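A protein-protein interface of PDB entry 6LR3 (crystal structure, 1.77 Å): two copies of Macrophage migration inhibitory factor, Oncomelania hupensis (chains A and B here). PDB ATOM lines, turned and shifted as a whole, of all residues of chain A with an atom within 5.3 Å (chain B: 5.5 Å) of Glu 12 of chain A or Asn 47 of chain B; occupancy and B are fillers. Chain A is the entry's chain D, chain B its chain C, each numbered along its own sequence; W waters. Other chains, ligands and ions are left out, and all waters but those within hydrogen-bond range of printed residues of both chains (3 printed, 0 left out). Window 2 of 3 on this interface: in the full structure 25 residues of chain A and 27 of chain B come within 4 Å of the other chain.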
ATOM      1  N   VAL A  10      11.564   4.479  12.370  1.00  0.00           N
ATOM      2  CA  VAL A  10      10.518   4.629  11.323  1.00  0.00           C
ATOM      3  C   VAL A  10       9.135   4.516  11.965  1.00  0.00           C
ATOM      4  O   VAL A  10       8.911   3.622  12.741  1.00  0.00           O
ATOM      5  CB  VAL A  10      10.729   3.630  10.171  1.00  0.00           C
ATOM      6  CG1 VAL A  10       9.568   3.639   9.173  1.00  0.00           C
ATOM      7  CG2 VAL A  10      12.071   3.930   9.504  1.00  0.00           C
ATOM      8  N   ALA A  11       8.242   5.415  11.637  1.00  0.00           N
ATOM      9  CA  ALA A  11       6.867   5.469  12.196  1.00  0.00           C
ATOM     10  C   ALA A  11       6.035   4.292  11.681  1.00  0.00           C
ATOM     11  O   ALA A  11       6.147   3.906  10.504  1.00  0.00           O
ATOM     12  CB  ALA A  11       6.221   6.784  11.893  1.00  0.00           C
ATOM     13  N   GLU A  12       5.181   3.766  12.548  1.00  0.00           N
ATOM     14  CA  GLU A  12       4.275   2.627  12.254  1.00  0.00           C
ATOM     15  C   GLU A  12       3.467   2.930  10.991  1.00  0.00           C
ATOM     16  O   GLU A  12       3.318   2.044  10.121  1.00  0.00           O
ATOM     17  CB  GLU A  12       3.358   2.384  13.454  1.00  0.00           C
ATOM     18  CG  GLU A  12       2.588   1.073  13.408  1.00  0.00           C
ATOM     19  CD  GLU A  12       1.817   0.813  14.705  1.00  0.00           C
ATOM     20  OE1 GLU A  12       2.128  -0.173  15.410  1.00  0.00           O
ATOM     21  OE2 GLU A  12       0.914   1.619  15.035  1.00  0.00           O
ATOM     22  N   LYS A  13       2.990   4.169  10.871  1.00  0.00           N
ATOM     23  CA  LYS A  13       2.092   4.550   9.755  1.00  0.00           C
ATOM     24  C   LYS A  13       2.839   4.444   8.429  1.00  0.00           C
ATOM     25  O   LYS A  13       2.139   4.321   7.405  1.00  0.00           O
ATOM     26  CB  LYS A  13       1.524   5.956   9.959  1.00  0.00           C
ATOM     27  CG  LYS A  13       2.535   7.089   9.818  1.00  0.00           C
ATOM     28  CD  LYS A  13       1.915   8.447  10.157  1.00  0.00           C
ATOM     29  CE  LYS A  13       2.726   9.620   9.646  1.00  0.00           C
ATOM     30  NZ  LYS A  13       4.117   9.589  10.166  1.00  0.00           N
ATOM     31  N   SER A  14       4.174   4.486   8.423  1.00  0.00           N
ATOM     32  CA  SER A  14       5.017   4.428   7.209  1.00  0.00           C
ATOM     33  C   SER A  14       5.236   2.988   6.750  1.00  0.00           C
ATOM     34  O   SER A  14       5.765   2.820   5.665  1.00  0.00           O
ATOM     35  CB  SER A  14       6.359   5.080   7.449  1.00  0.00           C
ATOM     36  OG  SER A  14       6.134   6.447   7.780  1.00  0.00           O
ATOM     37  N   ILE A  15       4.909   2.002   7.582  1.00  0.00           N
ATOM     38  CA  ILE A  15       5.291   0.593   7.344  1.00  0.00           C
ATOM     39  C   ILE A  15       4.127  -0.144   6.701  1.00  0.00           C
ATOM     40  O   ILE A  15       3.002  -0.093   7.187  1.00  0.00           O
ATOM     41  CB  ILE A  15       5.726  -0.048   8.668  1.00  0.00           C
ATOM     42  CG1 ILE A  15       6.894   0.749   9.259  1.00  0.00           C
ATOM     43  CG2 ILE A  15       6.014  -1.528   8.497  1.00  0.00           C
ATOM     44  CD1 ILE A  15       7.357   0.221  10.614  1.00  0.00           C
ATOM     45  N   GLN A  20       5.120  -7.359   8.790  1.00  0.00           N
ATOM     46  CA  GLN A  20       5.426  -8.405   9.791  1.00  0.00           C
ATOM     47  C   GLN A  20       5.078  -9.787   9.232  1.00  0.00           C
ATOM     48  O   GLN A  20       5.842 -10.731   9.495  1.00  0.00           O
ATOM     49  CB  GLN A  20       4.699  -8.170  11.101  1.00  0.00           C
ATOM     50  CG  GLN A  20       5.336  -7.115  11.955  1.00  0.00           C
ATOM     51  CD  GLN A  20       4.366  -6.673  13.014  1.00  0.00           C
ATOM     52  OE1 GLN A  20       3.447  -5.939  12.690  1.00  0.00           O
ATOM     53  NE2 GLN A  20       4.529  -7.126  14.256  1.00  0.00           N
ATOM     54  N   VAL A  40       7.414 -11.922  15.270  1.00  0.00           N
ATOM     55  CA  VAL A  40       8.013 -10.654  14.813  1.00  0.00           C
ATOM     56  C   VAL A  40       7.474  -9.570  15.740  1.00  0.00           C
ATOM     57  O   VAL A  40       6.265  -9.322  15.763  1.00  0.00           O
ATOM     58  CB  VAL A  40       7.738 -10.357  13.331  1.00  0.00           C
ATOM     59  CG1 VAL A  40       8.327  -9.013  12.960  1.00  0.00           C
ATOM     60  CG2 VAL A  40       8.246 -11.470  12.443  1.00  0.00           C
ATOM     61  N   ASP A  41       8.386  -8.988  16.494  1.00  0.00           N
ATOM     62  CA  ASP A  41       8.123  -7.936  17.496  1.00  0.00           C
ATOM     63  C   ASP A  41       8.648  -6.649  16.867  1.00  0.00           C
ATOM     64  O   ASP A  41       9.877  -6.451  16.811  1.00  0.00           O
ATOM     65  CB  ASP A  41       8.780  -8.318  18.817  1.00  0.00           C
ATOM     66  CG  ASP A  41       8.526  -7.368  19.959  1.00  0.00           C
ATOM     67  OD1 ASP A  41       7.899  -6.338  19.698  1.00  0.00           O
ATOM     68  OD2 ASP A  41       8.976  -7.683  21.082  1.00  0.00           O
ATOM     69  N   LEU A  42       7.725  -5.844  16.330  1.00  0.00           N
ATOM     70  CA  LEU A  42       8.084  -4.610  15.602  1.00  0.00           C
ATOM     71  C   LEU A  42       7.962  -3.451  16.570  1.00  0.00           C
ATOM     72  O   LEU A  42       6.829  -3.150  17.025  1.00  0.00           O
ATOM     73  CB  LEU A  42       7.177  -4.456  14.382  1.00  0.00           C
ATOM     74  CG  LEU A  42       7.323  -3.132  13.633  1.00  0.00           C
ATOM     75  CD1 LEU A  42       8.743  -2.922  13.150  1.00  0.00           C
ATOM     76  CD2 LEU A  42       6.356  -3.119  12.457  1.00  0.00           C
ATOM     77  N   SER A  44       8.254   0.090  16.211  1.00  0.00           N
ATOM     78  CA  SER A  44       8.306   1.227  15.300  1.00  0.00           C
ATOM     79  C   SER A  44       8.088   2.502  16.108  1.00  0.00           C
ATOM     80  O   SER A  44       7.570   2.452  17.235  1.00  0.00           O
ATOM     81  CB  SER A  44       7.335   1.001  14.175  1.00  0.00           C
ATOM     82  OG  SER A  44       6.056   0.960  14.723  1.00  0.00           O
ATOM     83  N   GLY A  45       8.525   3.612  15.545  1.00  0.00           N
ATOM     84  CA  GLY A  45       8.536   4.928  16.205  1.00  0.00           C
ATOM     85  C   GLY A  45       9.295   4.838  17.518  1.00  0.00           C
ATOM     86  O   GLY A  45       9.023   5.635  18.420  1.00  0.00           O
ATOM     87  N   GLY B  45       0.368  -4.312  24.882  1.00  0.00           N
ATOM     88  CA  GLY B  45      -0.115  -3.716  23.625  1.00  0.00           C
ATOM     89  C   GLY B  45       1.020  -3.633  22.627  1.00  0.00           C
ATOM     90  O   GLY B  45       0.976  -2.764  21.730  1.00  0.00           O
ATOM     91  N   ALA B  46       2.004  -4.508  22.746  1.00  0.00           N
ATOM     92  CA  ALA B  46       3.179  -4.531  21.862  1.00  0.00           C
ATOM     93  C   ALA B  46       2.750  -5.003  20.481  1.00  0.00           C
ATOM     94  O   ALA B  46       1.805  -5.814  20.376  1.00  0.00           O
ATOM     95  CB  ALA B  46       4.279  -5.360  22.439  1.00  0.00           C
ATOM     96  N   ASN B  47       3.440  -4.518  19.455  1.00  0.00           N
ATOM     97  CA  ASN B  47       3.186  -4.985  18.074  1.00  0.00           C
ATOM     98  C   ASN B  47       3.985  -6.259  17.844  1.00  0.00           C
ATOM     99  O   ASN B  47       4.972  -6.246  17.096  1.00  0.00           O
ATOM    100  CB  ASN B  47       3.489  -3.917  17.045  1.00  0.00           C
ATOM    101  CG  ASN B  47       2.976  -4.365  15.703  1.00  0.00           C
ATOM    102  OD1 ASN B  47       2.394  -5.454  15.576  1.00  0.00           O
ATOM    103  ND2 ASN B  47       3.226  -3.553  14.692  1.00  0.00           N
ATOM    104  N   ILE B  48       3.575  -7.320  18.521  1.00  0.00           N
ATOM    105  CA  ILE B  48       4.230  -8.632  18.435  1.00  0.00           C
ATOM    106  C   ILE B  48       3.204  -9.616  17.885  1.00  0.00           C
ATOM    107  O   ILE B  48       2.075  -9.696  18.402  1.00  0.00           O
ATOM    108  CB  ILE B  48       4.844  -9.057  19.781  1.00  0.00           C
ATOM    109  CG1 ILE B  48       5.577 -10.383  19.631  1.00  0.00           C
ATOM    110  CG2 ILE B  48       3.819  -9.103  20.926  1.00  0.00           C
ATOM    111  CD1 ILE B  48       6.456 -10.676  20.846  1.00  0.00           C
ATOM    112  N   MET B  49       3.570 -10.225  16.766  1.00  0.00           N
ATOM    113  CA  MET B  49       2.755 -11.280  16.154  1.00  0.00           C
ATOM    114  C   MET B  49       3.508 -12.592  16.284  1.00  0.00           C
ATOM    115  O   MET B  49       4.754 -12.598  16.411  1.00  0.00           O
ATOM    116  CB  MET B  49       2.328 -10.951  14.729  1.00  0.00           C
ATOM    117  CG  MET B  49       3.364 -11.061  13.709  1.00  0.00           C
ATOM    118  SD  MET B  49       2.689 -11.255  11.957  1.00  0.00           S
ATOM    119  CE  MET B  49       1.496  -9.928  11.894  1.00  0.00           C
ATOM    120  N   ARG B  54      -2.359 -12.424  15.018  1.00  0.00           N
ATOM    121  CA  ARG B  54      -2.373 -11.449  16.118  1.00  0.00           C
ATOM    122  C   ARG B  54      -3.241 -11.964  17.259  1.00  0.00           C
ATOM    123  O   ARG B  54      -3.622 -11.149  18.102  1.00  0.00           O
ATOM    124  CB  ARG B  54      -2.783 -10.091  15.566  1.00  0.00           C
ATOM    125  CG  ARG B  54      -1.814  -9.568  14.514  1.00  0.00           C
ATOM    126  CD  ARG B  54      -2.126  -8.152  14.197  1.00  0.00           C
ATOM    127  NE  ARG B  54      -1.216  -7.535  13.244  1.00  0.00           N
ATOM    128  CZ  ARG B  54      -0.030  -7.027  13.544  1.00  0.00           C
ATOM    129  NH1 ARG B  54       0.444  -7.125  14.767  1.00  0.00           N
ATOM    130  NH2 ARG B  54       0.691  -6.438  12.618  1.00  0.00           N
HETATM  131  O   HOH W   1       2.056  -3.221  12.069  1.00  0.00           O
HETATM  132  O   HOH W   2       6.328  -3.942  19.670  1.00  0.00           O
HETATM  133  O   HOH W   3       4.668  -1.148  15.407  1.00  0.00           O
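The backbone carbonyl oxygen of Asn 47 of chain B sits at hydrogen-bond distance from the side-chain amide nitrogen of Gln 20 of chain A (3.0 Å).
The backbone carbonyl oxygen (O) of Asn 47 of chain B sits at hydrogen-bond distance from the backbone NH (N) of Leu 42 of chain A (2.9 Å).
N of Val 40 of chain A lies within hydrogen-bond range of O of Met 49 of chain B.
The guanidinium group of Arg 54 of chain B lies within hydrogen-bond range of the side-chain amide oxygen of Gln 20 of chain A (2.8 Å).
Glu 12 of chain A touches one residue of chain B.
Printed residues of chain B within 4 Å of Gln 20 of chain A: Asn 47, Met 49 and Arg 54.
Of the printed residues of chain B, Asp 41 of chain A touches Asn 47 (3.6 Å) and Ile 48 (3.9 Å).
Printed residues of chain B within 4 Å of Leu 42 of chain A: Asn 47 (2.9 Å).
Gly 45 of chain A touches none of the printed residues of chain B.
Asn 47 of chain B touches just these residues of chain A: Glu 12, Gln 20, Val 40, Asp 41 and Leu 42.
Of the printed residues of chain A, Ile 48 of chain B touches Val 40 (3.4 Å) and Asp 41 (3.9 Å).
Printed residues of chain A within 4 Å of Met 49 of chain B: Gln 20 and Val 40.
The nearest printed residue of chain B that does not touch Glu 12 of chain A is Gly 45 of chain B (6.9 Å).
The nearest printed residue of chain A that does not touch Asn 47 of chain B is Ser 44 of chain A (5.3 Å).
Among the printed residues, pairs that only touch across the chains: Glu 12 of chain A with Asn 47 of chain B (3.6 Å), Gln 20 of chain A with Met 49 of chain B (3.7 Å), Val 40 of chain A with Asn 47 of chain B (3.6 Å), Val 40 of chain A with Ile 48 of chain B (3.4 Å), Asp 41 of chain A with Asn 47 of chain B (3.6 Å) and Asp 41 of chain A with Ile 48 of chain B (3.9 Å).
Water W3 lies within hydrogen-bond range of OG of Ser 44 of chain A (2.6 Å), OE1 of Glu 12 of chain A (2.7 Å), ND2 of Asn 47 of chain B (2.9 Å) and O of Leu 42 of chain A (3.4 Å).
Water W2 lies within hydrogen-bond range of O of Leu 42 of chain A (2.8 Å), OD1 of Asp 41 of chain A (2.9 Å) and N of Asn 47 of chain B (3.0 Å).
Water W1 lies within hydrogen-bond range of ND2 of Asn 47 of chain B (2.9 Å) and OE1 of Gln 20 of chain A (3.1 Å).
The side-chain amide oxygen (OD1) of Asn 47 of chain B is in hydrogen-bond range of the guanidinium group (NH1) of Arg 54 of chain B (2.7 Å).
The side-chain amide nitrogen (NE2) of Gln 20 of chain A lies within hydrogen-bond range of the backbone carbonyl oxygen (O) of Val 40 of chain A (3.2 Å).
Of the 6 printed residues of chain B, 4 touch a printed residue of chain A.
Printed residues of chain B that touch a printed residue of chain A: Asn 47, Ile 48, Met 49 and Arg 54.
Hydrophobic or aromatic side chains of chain B that line the printed part of chain A: Ile 48 and Met 49.
Of the 12 printed residues of chain A, 5 touch a printed residue of chain B.
Hydrophobic or aromatic side chains of chain A that line the printed part of chain B: Leu 42.
Position printed for both chains: 45.
Of the 10 pairs that touch across the chains among the printed residues, none has its exchanged pair printed and touching as well.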
